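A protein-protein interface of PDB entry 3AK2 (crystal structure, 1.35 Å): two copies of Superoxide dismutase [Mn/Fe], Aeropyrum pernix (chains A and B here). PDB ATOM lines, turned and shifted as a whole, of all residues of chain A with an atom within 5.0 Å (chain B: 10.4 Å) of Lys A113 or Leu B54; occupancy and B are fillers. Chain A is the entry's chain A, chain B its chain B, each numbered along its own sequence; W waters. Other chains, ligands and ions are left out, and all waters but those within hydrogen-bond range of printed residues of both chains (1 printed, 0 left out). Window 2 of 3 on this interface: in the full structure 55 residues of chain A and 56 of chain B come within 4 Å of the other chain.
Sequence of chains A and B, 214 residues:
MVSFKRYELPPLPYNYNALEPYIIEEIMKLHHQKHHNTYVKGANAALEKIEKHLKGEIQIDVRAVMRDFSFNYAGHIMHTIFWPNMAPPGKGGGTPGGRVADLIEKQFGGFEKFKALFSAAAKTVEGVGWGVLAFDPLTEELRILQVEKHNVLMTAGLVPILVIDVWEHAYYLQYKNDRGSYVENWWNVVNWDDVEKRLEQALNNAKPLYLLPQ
O of Leu B54 is in hydrogen-bond range of NZ of Lys A113 (2.9 Å).
Among the printed residues, merely in contact across the chains: Gln A107 with Leu B54 (3.9998 Å), Phe A108 with Leu B54 (3.7 Å), Leu A117 with Ile B50 (3.9 Å), Leu A117 with Leu B54 (3.9 Å), Leu A117 with Val B62 (3.9 Å) and Leu A117 with Met B66 (3.97 Å).
Printed residues of chain B within 4 Å of Phe A108: Leu B54 (3.7 Å).
Gly A110 touches none of the printed residues of chain B.
Lys A113 touches just one residue of chain B: Leu B54 (2.9 Å).
Printed residues of chain A within 4 Å of Ile B50: Leu A117.
Of the printed residues of chain A, Leu B54 touches Gln A107, Phe A108, Lys A113 and Leu A117.
Of the printed residues of chain A, Val B62 touches Leu A117.
Of the printed residues of chain A, Met B66 touches Leu A117.
Of the 11 printed residues of chain A, 4 touch a printed residue of chain B.
Of the 20 printed residues of chain B, 4 touch a printed residue of chain A.
No position is printed for both chains.
Of the 7 pairs that touch across the chains among the printed residues, none has its exchanged pair printed and touching as well.
Water W1 bridges a ring nitrogen (NE2) of His B53 (2.7 Å) and the backbone NH of Leu A117 (3.5 Å).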
ATOM      1  N   GLN A 107      27.919 -13.483 -15.559  1.00  0.00           N
ATOM      2  CA  GLN A 107      27.572 -13.498 -14.142  1.00  0.00           C
ATOM      3  C   GLN A 107      28.198 -14.631 -13.356  1.00  0.00           C
ATOM      4  O   GLN A 107      28.638 -14.429 -12.221  1.00  0.00           O
ATOM      5  CB  GLN A 107      26.066 -13.556 -13.979  1.00  0.00           C
ATOM      6  CG  GLN A 107      25.358 -12.394 -14.614  1.00  0.00           C
ATOM      7  CD  GLN A 107      23.893 -12.434 -14.323  1.00  0.00           C
ATOM      8  OE1 GLN A 107      23.070 -12.472 -15.235  1.00  0.00           O
ATOM      9  NE2 GLN A 107      23.550 -12.457 -13.038  1.00  0.00           N
ATOM     10  N   PHE A 108      28.221 -15.821 -13.947  1.00  0.00           N
ATOM     11  CA  PHE A 108      28.694 -17.004 -13.237  1.00  0.00           C
ATOM     12  C   PHE A 108      30.090 -17.430 -13.673  1.00  0.00           C
ATOM     13  O   PHE A 108      30.665 -18.349 -13.097  1.00  0.00           O
ATOM     14  CB  PHE A 108      27.692 -18.158 -13.369  1.00  0.00           C
ATOM     15  CG  PHE A 108      26.304 -17.806 -12.907  1.00  0.00           C
ATOM     16  CD1 PHE A 108      26.020 -17.660 -11.551  1.00  0.00           C
ATOM     17  CD2 PHE A 108      25.281 -17.610 -13.827  1.00  0.00           C
ATOM     18  CE1 PHE A 108      24.739 -17.326 -11.120  1.00  0.00           C
ATOM     19  CE2 PHE A 108      23.994 -17.276 -13.405  1.00  0.00           C
ATOM     20  CZ  PHE A 108      23.724 -17.132 -12.048  1.00  0.00           C
ATOM     21  N   GLY A 109      30.633 -16.748 -14.679  1.00  0.00           N
ATOM     22  CA  GLY A 109      31.956 -17.070 -15.204  1.00  0.00           C
ATOM     23  C   GLY A 109      31.949 -18.294 -16.103  1.00  0.00           C
ATOM     24  O   GLY A 109      32.941 -19.020 -16.185  1.00  0.00           O
ATOM     25  N   GLY A 110      30.826 -18.528 -16.776  1.00  0.00           N
ATOM     26  CA  GLY A 110      30.730 -19.610 -17.752  1.00  0.00           C
ATOM     27  C   GLY A 110      29.825 -20.753 -17.338  1.00  0.00           C
ATOM     28  O   GLY A 110      29.401 -20.842 -16.177  1.00  0.00           O
ATOM     29  N   PHE A 111      29.538 -21.636 -18.289  1.00  0.00           N
ATOM     30  CA  PHE A 111      28.561 -22.701 -18.073  1.00  0.00           C
ATOM     31  C   PHE A 111      28.938 -23.701 -16.983  1.00  0.00           C
ATOM     32  O   PHE A 111      28.085 -24.090 -16.187  1.00  0.00           O
ATOM     33  CB  PHE A 111      28.221 -23.438 -19.373  1.00  0.00           C
ATOM     34  CG  PHE A 111      27.179 -24.500 -19.186  1.00  0.00           C
ATOM     35  CD1 PHE A 111      25.850 -24.147 -18.984  1.00  0.00           C
ATOM     36  CD2 PHE A 111      27.525 -25.847 -19.161  1.00  0.00           C
ATOM     37  CE1 PHE A 111      24.878 -25.115 -18.788  1.00  0.00           C
ATOM     38  CE2 PHE A 111      26.558 -26.825 -18.964  1.00  0.00           C
ATOM     39  CZ  PHE A 111      25.232 -26.457 -18.777  1.00  0.00           C
ATOM     40  N   GLU A 112      30.198 -24.123 -16.940  1.00  0.00           N
ATOM     41  CA  GLU A 112      30.609 -25.105 -15.937  1.00  0.00           C
ATOM     42  C   GLU A 112      30.509 -24.567 -14.506  1.00  0.00           C
ATOM     43  O   GLU A 112      30.070 -25.283 -13.604  1.00  0.00           O
ATOM     44  CB  GLU A 112      32.005 -25.670 -16.231  1.00  0.00           C
ATOM     45  CG  GLU A 112      32.096 -26.495 -17.521  1.00  0.00           C
ATOM     46  CD  GLU A 112      31.125 -27.676 -17.574  1.00  0.00           C
ATOM     47  OE1 GLU A 112      30.915 -28.347 -16.539  1.00  0.00           O
ATOM     48  OE2 GLU A 112      30.578 -27.939 -18.665  1.00  0.00           O
ATOM     49  N   LYS A 113      30.900 -23.311 -14.306  1.00  0.00           N
ATOM     50  CA  LYS A 113      30.761 -22.671 -12.996  1.00  0.00           C
ATOM     51  C   LYS A 113      29.287 -22.537 -12.599  1.00  0.00           C
ATOM     52  O   LYS A 113      28.922 -22.822 -11.455  1.00  0.00           O
ATOM     53  CB  LYS A 113      31.464 -21.312 -12.963  1.00  0.00           C
ATOM     54  CG  LYS A 113      32.988 -21.392 -12.862  1.00  0.00           C
ATOM     55  CD  LYS A 113      33.615 -20.003 -12.753  1.00  0.00           C
ATOM     56  CE  LYS A 113      35.140 -20.070 -12.701  1.00  0.00           C
ATOM     57  NZ  LYS A 113      35.626 -20.801 -11.496  1.00  0.00           N
ATOM     58  N   PHE A 114      28.449 -22.122 -13.551  1.00  0.00           N
ATOM     59  CA  PHE A 114      27.000 -22.052 -13.335  1.00  0.00           C
ATOM     60  C   PHE A 114      26.419 -23.422 -12.983  1.00  0.00           C
ATOM     61  O   PHE A 114      25.652 -23.553 -12.027  1.00  0.00           O
ATOM     62  CB  PHE A 114      26.283 -21.490 -14.568  1.00  0.00           C
ATOM     63  CG  PHE A 114      24.838 -21.912 -14.672  1.00  0.00           C
ATOM     64  CD1 PHE A 114      23.851 -21.254 -13.941  1.00  0.00           C
ATOM     65  CD2 PHE A 114      24.470 -22.987 -15.478  1.00  0.00           C
ATOM     66  CE1 PHE A 114      22.522 -21.657 -14.018  1.00  0.00           C
ATOM     67  CE2 PHE A 114      23.146 -23.398 -15.556  1.00  0.00           C
ATOM     68  CZ  PHE A 114      22.169 -22.727 -14.828  1.00  0.00           C
ATOM     69  N   LYS A 115      26.774 -24.435 -13.772  1.00  0.00           N
ATOM     70  CA  LYS A 115      26.238 -25.778 -13.594  1.00  0.00           C
ATOM     71  C   LYS A 115      26.584 -26.321 -12.209  1.00  0.00           C
ATOM     72  O   LYS A 115      25.732 -26.899 -11.529  1.00  0.00           O
ATOM     73  CB  LYS A 115      26.767 -26.712 -14.687  1.00  0.00           C
ATOM     74  CG  LYS A 115      26.252 -28.131 -14.580  1.00  0.00           C
ATOM     75  CD  LYS A 115      26.723 -28.986 -15.741  1.00  0.00           C
ATOM     76  CE  LYS A 115      26.310 -30.429 -15.548  1.00  0.00           C
ATOM     77  NZ  LYS A 115      26.758 -31.286 -16.680  1.00  0.00           N
ATOM     78  N   ALA A 116      27.829 -26.120 -11.788  1.00  0.00           N
ATOM     79  CA  ALA A 116      28.267 -26.572 -10.475  1.00  0.00           C
ATOM     80  C   ALA A 116      27.475 -25.891  -9.357  1.00  0.00           C
ATOM     81  O   ALA A 116      27.090 -26.539  -8.385  1.00  0.00           O
ATOM     82  CB  ALA A 116      29.764 -26.332 -10.301  1.00  0.00           C
ATOM     83  N   LEU A 117      27.225 -24.593  -9.499  1.00  0.00           N
ATOM     84  CA  LEU A 117      26.504 -23.849  -8.468  1.00  0.00           C
ATOM     85  C   LEU A 117      25.030 -24.235  -8.426  1.00  0.00           C
ATOM     86  O   LEU A 117      24.474 -24.471  -7.351  1.00  0.00           O
ATOM     87  CB  LEU A 117      26.661 -22.338  -8.669  1.00  0.00           C
ATOM     88  CG  LEU A 117      25.973 -21.430  -7.641  1.00  0.00           C
ATOM     89  CD1 LEU A 117      26.450 -21.725  -6.225  1.00  0.00           C
ATOM     90  CD2 LEU A 117      26.190 -19.966  -7.975  1.00  0.00           C
ATOM     91  N   ARG B   6      24.778  -4.668  -7.986  1.00  0.00           N
ATOM     92  CA  ARG B   6      24.409  -4.428  -6.593  1.00  0.00           C
ATOM     93  C   ARG B   6      23.100  -3.653  -6.454  1.00  0.00           C
ATOM     94  O   ARG B   6      22.726  -2.855  -7.324  1.00  0.00           O
ATOM     95  CB  ARG B   6      25.540  -3.713  -5.836  1.00  0.00           C
ATOM     96  CG  ARG B   6      26.865  -4.492  -5.737  1.00  0.00           C
ATOM     97  CD  ARG B   6      26.745  -5.743  -4.866  1.00  0.00           C
ATOM     98  NE  ARG B   6      28.049  -6.288  -4.478  1.00  0.00           N
ATOM     99  CZ  ARG B   6      28.661  -7.305  -5.080  1.00  0.00           C
ATOM    100  NH1 ARG B   6      28.101  -7.920  -6.115  1.00  0.00           N
ATOM    101  NH2 ARG B   6      29.846  -7.714  -4.642  1.00  0.00           N
ATOM    102  N   ALA B  46      25.385 -11.102   0.441  1.00  0.00           N
ATOM    103  CA  ALA B  46      25.179 -12.468  -0.035  1.00  0.00           C
ATOM    104  C   ALA B  46      25.725 -12.640  -1.451  1.00  0.00           C
ATOM    105  O   ALA B  46      26.393 -13.634  -1.744  1.00  0.00           O
ATOM    106  CB  ALA B  46      23.701 -12.842   0.033  1.00  0.00           C
ATOM    107  N   LEU B  47      25.465 -11.661  -2.316  1.00  0.00           N
ATOM    108  CA  LEU B  47      25.994 -11.683  -3.680  1.00  0.00           C
ATOM    109  C   LEU B  47      27.522 -11.666  -3.719  1.00  0.00           C
ATOM    110  O   LEU B  47      28.129 -12.345  -4.548  1.00  0.00           O
ATOM    111  CB  LEU B  47      25.439 -10.520  -4.508  1.00  0.00           C
ATOM    112  CG  LEU B  47      23.952 -10.549  -4.871  1.00  0.00           C
ATOM    113  CD1 LEU B  47      23.607  -9.304  -5.669  1.00  0.00           C
ATOM    114  CD2 LEU B  47      23.580 -11.809  -5.642  1.00  0.00           C
ATOM    115  N   GLU B  48      28.136 -10.889  -2.831  1.00  0.00           N
ATOM    116  CA  GLU B  48      29.598 -10.830  -2.739  1.00  0.00           C
ATOM    117  C   GLU B  48      30.185 -12.201  -2.397  1.00  0.00           C
ATOM    118  O   GLU B  48      31.198 -12.616  -2.971  1.00  0.00           O
ATOM    119  CB  GLU B  48      30.028  -9.779  -1.709  1.00  0.00           C
ATOM    120  CG  GLU B  48      31.541  -9.586  -1.581  1.00  0.00           C
ATOM    121  CD  GLU B  48      31.924  -8.493  -0.593  1.00  0.00           C
ATOM    122  OE1 GLU B  48      31.253  -8.357   0.455  1.00  0.00           O
ATOM    123  OE2 GLU B  48      32.909  -7.773  -0.863  1.00  0.00           O
ATOM    124  N   LYS B  49      29.538 -12.902  -1.472  1.00  0.00           N
ATOM    125  CA  LYS B  49      29.946 -14.254  -1.098  1.00  0.00           C
ATOM    126  C   LYS B  49      29.817 -15.234  -2.269  1.00  0.00           C
ATOM    127  O   LYS B  49      30.711 -16.051  -2.505  1.00  0.00           O
ATOM    128  CB  LYS B  49      29.147 -14.745   0.113  1.00  0.00           C
ATOM    129  CG  LYS B  49      29.478 -14.022   1.417  1.00  0.00           C
ATOM    130  CD  LYS B  49      28.461 -14.338   2.501  1.00  0.00           C
ATOM    131  CE  LYS B  49      28.655 -13.438   3.704  1.00  0.00           C
ATOM    132  NZ  LYS B  49      27.659 -13.739   4.770  1.00  0.00           N
ATOM    133  N   ILE B  50      28.714 -15.141  -3.009  1.00  0.00           N
ATOM    134  CA  ILE B  50      28.515 -15.995  -4.176  1.00  0.00           C
ATOM    135  C   ILE B  50      29.596 -15.710  -5.224  1.00  0.00           C
ATOM    136  O   ILE B  50      30.142 -16.641  -5.824  1.00  0.00           O
ATOM    137  CB  ILE B  50      27.077 -15.868  -4.748  1.00  0.00           C
ATOM    138  CG1 ILE B  50      26.060 -16.375  -3.714  1.00  0.00           C
ATOM    139  CG2 ILE B  50      26.927 -16.668  -6.043  1.00  0.00           C
ATOM    140  CD1 ILE B  50      24.606 -16.022  -4.014  1.00  0.00           C
ATOM    141  N   GLU B  51      29.926 -14.432  -5.407  1.00  0.00           N
ATOM    142  CA  GLU B  51      30.991 -14.031  -6.328  1.00  0.00           C
ATOM    143  C   GLU B  51      32.330 -14.667  -5.955  1.00  0.00           C
ATOM    144  O   GLU B  51      33.004 -15.252  -6.805  1.00  0.00           O
ATOM    145  CB  GLU B  51      31.131 -12.512  -6.364  1.00  0.00           C
ATOM    146  CG  GLU B  51      30.040 -11.807  -7.149  1.00  0.00           C
ATOM    147  CD  GLU B  51      30.466 -10.443  -7.659  1.00  0.00           C
ATOM    148  OE1 GLU B  51      31.673 -10.248  -7.922  1.00  0.00           O
ATOM    149  OE2 GLU B  51      29.587  -9.568  -7.812  1.00  0.00           O
ATOM    150  N   LYS B  52      32.708 -14.552  -4.684  1.00  0.00           N
ATOM    151  CA  LYS B  52      33.973 -15.114  -4.208  1.00  0.00           C
ATOM    152  C   LYS B  52      33.999 -16.635  -4.367  1.00  0.00           C
ATOM    153  O   LYS B  52      35.038 -17.215  -4.691  1.00  0.00           O
ATOM    154  CB  LYS B  52      34.239 -14.706  -2.754  1.00  0.00           C
ATOM    155  CG  LYS B  52      34.526 -13.221  -2.549  1.00  0.00           C
ATOM    156  CD  LYS B  52      34.803 -12.911  -1.078  1.00  0.00           C
ATOM    157  CE  LYS B  52      34.991 -11.416  -0.835  1.00  0.00           C
ATOM    158  NZ  LYS B  52      36.253 -10.889  -1.428  1.00  0.00           N
ATOM    159  N   HIS B  53      32.849 -17.269  -4.156  1.00  0.00           N
ATOM    160  CA  HIS B  53      32.692 -18.705  -4.354  1.00  0.00           C
ATOM    161  C   HIS B  53      32.907 -19.101  -5.820  1.00  0.00           C
ATOM    162  O   HIS B  53      33.654 -20.037  -6.112  1.00  0.00           O
ATOM    163  CB  HIS B  53      31.304 -19.143  -3.874  1.00  0.00           C
ATOM    164  CG  HIS B  53      31.009 -20.589  -4.110  1.00  0.00           C
ATOM    165  ND1 HIS B  53      31.298 -21.570  -3.185  1.00  0.00           N
ATOM    166  CD2 HIS B  53      30.450 -21.222  -5.169  1.00  0.00           C
ATOM    167  CE1 HIS B  53      30.930 -22.744  -3.665  1.00  0.00           C
ATOM    168  NE2 HIS B  53      30.412 -22.561  -4.865  1.00  0.00           N
ATOM    169  N   LEU B  54      32.257 -18.379  -6.731  1.00  0.00           N
ATOM    170  CA  LEU B  54      32.368 -18.639  -8.170  1.00  0.00           C
ATOM    171  C   LEU B  54      33.779 -18.406  -8.706  1.00  0.00           C
ATOM    172  O   LEU B  54      34.231 -19.119  -9.607  1.00  0.00           O
ATOM    173  CB  LEU B  54      31.370 -17.777  -8.944  1.00  0.00           C
ATOM    174  CG  LEU B  54      29.904 -18.203  -8.851  1.00  0.00           C
ATOM    175  CD1 LEU B  54      29.007 -17.036  -9.210  1.00  0.00           C
ATOM    176  CD2 LEU B  54      29.621 -19.411  -9.741  1.00  0.00           C
ATOM    177  N   LYS B  55      34.468 -17.415  -8.150  1.00  0.00           N
ATOM    178  CA  LYS B  55      35.857 -17.134  -8.516  1.00  0.00           C
ATOM    179  C   LYS B  55      36.824 -18.145  -7.894  1.00  0.00           C
ATOM    180  O   LYS B  55      38.017 -18.149  -8.213  1.00  0.00           O
ATOM    181  CB  LYS B  55      36.243 -15.715  -8.099  1.00  0.00           C
ATOM    182  CG  LYS B  55      35.520 -14.612  -8.853  1.00  0.00           C
ATOM    183  CD  LYS B  55      35.949 -13.253  -8.330  1.00  0.00           C
ATOM    184  CE  LYS B  55      35.077 -12.137  -8.877  1.00  0.00           C
ATOM    185  NZ  LYS B  55      35.512 -10.814  -8.349  1.00  0.00           N
ATOM    186  N   GLY B  56      36.306 -18.992  -7.006  1.00  0.00           N
ATOM    187  CA  GLY B  56      37.098 -20.028  -6.344  1.00  0.00           C
ATOM    188  C   GLY B  56      37.959 -19.522  -5.200  1.00  0.00           C
ATOM    189  O   GLY B  56      38.875 -20.216  -4.753  1.00  0.00           O
ATOM    190  N   GLU B  57      37.658 -18.318  -4.718  1.00  0.00           N
ATOM    191  CA  GLU B  57      38.420 -17.678  -3.640  1.00  0.00           C
ATOM    192  C   GLU B  57      38.019 -18.201  -2.264  1.00  0.00           C
ATOM    193  O   GLU B  57      38.848 -18.298  -1.357  1.00  0.00           O
ATOM    194  CB  GLU B  57      38.272 -16.156  -3.713  1.00  0.00           C
ATOM    195  CG  GLU B  57      38.917 -15.558  -4.964  1.00  0.00           C
ATOM    196  CD  GLU B  57      38.496 -14.129  -5.258  1.00  0.00           C
ATOM    197  OE1 GLU B  57      38.916 -13.603  -6.310  1.00  0.00           O
ATOM    198  OE2 GLU B  57      37.750 -13.529  -4.455  1.00  0.00           O
ATOM    199  N   ILE B  58      36.735 -18.521  -2.120  1.00  0.00           N
ATOM    200  CA  ILE B  58      36.204 -19.161  -0.917  1.00  0.00           C
ATOM    201  C   ILE B  58      35.257 -20.280  -1.341  1.00  0.00           C
ATOM    202  O   ILE B  58      34.884 -20.377  -2.512  1.00  0.00           O
ATOM    203  CB  ILE B  58      35.443 -18.161   0.014  1.00  0.00           C
ATOM    204  CG1 ILE B  58      34.179 -17.617  -0.671  1.00  0.00           C
ATOM    205  CG2 ILE B  58      36.363 -17.033   0.501  1.00  0.00           C
ATOM    206  CD1 ILE B  58      33.316 -16.707   0.207  1.00  0.00           C
ATOM    207  N   GLN B  59      34.884 -21.132  -0.392  1.00  0.00           N
ATOM    208  CA  GLN B  59      33.773 -22.053  -0.591  1.00  0.00           C
ATOM    209  C   GLN B  59      32.685 -21.729   0.416  1.00  0.00           C
ATOM    210  O   GLN B  59      32.928 -21.710   1.624  1.00  0.00           O
ATOM    211  CB  GLN B  59      34.217 -23.511  -0.461  1.00  0.00           C
ATOM    212  CG  GLN B  59      34.768 -24.103  -1.752  1.00  0.00           C
ATOM    213  CD  GLN B  59      34.333 -25.546  -1.953  1.00  0.00           C
ATOM    214  OE1 GLN B  59      33.520 -25.842  -2.831  1.00  0.00           O
ATOM    215  NE2 GLN B  59      34.863 -26.449  -1.134  1.00  0.00           N
ATOM    216  N   ILE B  60      31.488 -21.457  -0.091  1.00  0.00           N
ATOM    217  CA  ILE B  60      30.369 -21.079   0.767  1.00  0.00           C
ATOM    218  C   ILE B  60      29.437 -22.252   1.025  1.00  0.00           C
ATOM    219  O   ILE B  60      29.426 -23.227   0.269  1.00  0.00           O
ATOM    220  CB  ILE B  60      29.551 -19.891   0.175  1.00  0.00           C
ATOM    221  CG1 ILE B  60      28.864 -20.286  -1.145  1.00  0.00           C
ATOM    222  CG2 ILE B  60      30.431 -18.659   0.017  1.00  0.00           C
ATOM    223  CD1 ILE B  60      27.965 -19.216  -1.740  1.00  0.00           C
ATOM    224  N   ASP B  61      28.667 -22.152   2.108  1.00  0.00           N
ATOM    225  CA  ASP B  61      27.493 -22.988   2.290  1.00  0.00           C
ATOM    226  C   ASP B  61      26.442 -22.380   1.370  1.00  0.00           C
ATOM    227  O   ASP B  61      25.882 -21.319   1.662  1.00  0.00           O
ATOM    228  CB  ASP B  61      27.033 -22.976   3.753  1.00  0.00           C
ATOM    229  CG  ASP B  61      25.757 -23.787   3.989  1.00  0.00           C
ATOM    230  OD1 ASP B  61      24.946 -23.956   3.059  1.00  0.00           O
ATOM    231  OD2 ASP B  61      25.556 -24.246   5.131  1.00  0.00           O
ATOM    232  N   VAL B  62      26.201 -23.046   0.248  1.00  0.00           N
ATOM    233  CA  VAL B  62      25.336 -22.518  -0.800  1.00  0.00           C
ATOM    234  C   VAL B  62      23.910 -22.303  -0.279  1.00  0.00           C
ATOM    235  O   VAL B  62      23.304 -21.257  -0.516  1.00  0.00           O
ATOM    236  CB  VAL B  62      25.377 -23.428  -2.056  1.00  0.00           C
ATOM    237  CG1 VAL B  62      24.333 -23.021  -3.070  1.00  0.00           C
ATOM    238  CG2 VAL B  62      26.768 -23.389  -2.688  1.00  0.00           C
ATOM    239  N   VAL B  65      23.882 -19.173   2.224  1.00  0.00           N
ATOM    240  CA  VAL B  65      24.037 -17.888   1.555  1.00  0.00           C
ATOM    241  C   VAL B  65      22.815 -17.569   0.681  1.00  0.00           C
ATOM    242  O   VAL B  65      22.389 -16.417   0.597  1.00  0.00           O
ATOM    243  CB  VAL B  65      25.364 -17.808   0.760  1.00  0.00           C
ATOM    244  CG1 VAL B  65      25.476 -16.486   0.021  1.00  0.00           C
ATOM    245  CG2 VAL B  65      26.547 -17.969   1.710  1.00  0.00           C
ATOM    246  N   MET B  66      22.232 -18.583   0.052  1.00  0.00           N
ATOM    247  CA  MET B  66      21.003 -18.355  -0.706  1.00  0.00           C
ATOM    248  C   MET B  66      19.803 -18.025   0.185  1.00  0.00           C
ATOM    249  O   MET B  66      18.966 -17.214  -0.194  1.00  0.00           O
ATOM    250  CB  MET B  66      20.719 -19.491  -1.680  1.00  0.00           C
ATOM    251  CG  MET B  66      21.669 -19.442  -2.849  1.00  0.00           C
ATOM    252  SD  MET B  66      21.543 -20.855  -3.938  1.00  0.00           S
ATOM    253  CE  MET B  66      22.868 -20.447  -5.070  1.00  0.00           C
HETATM  254  O   HOH W   1      29.461 -24.201  -6.843  1.00  0.00           O
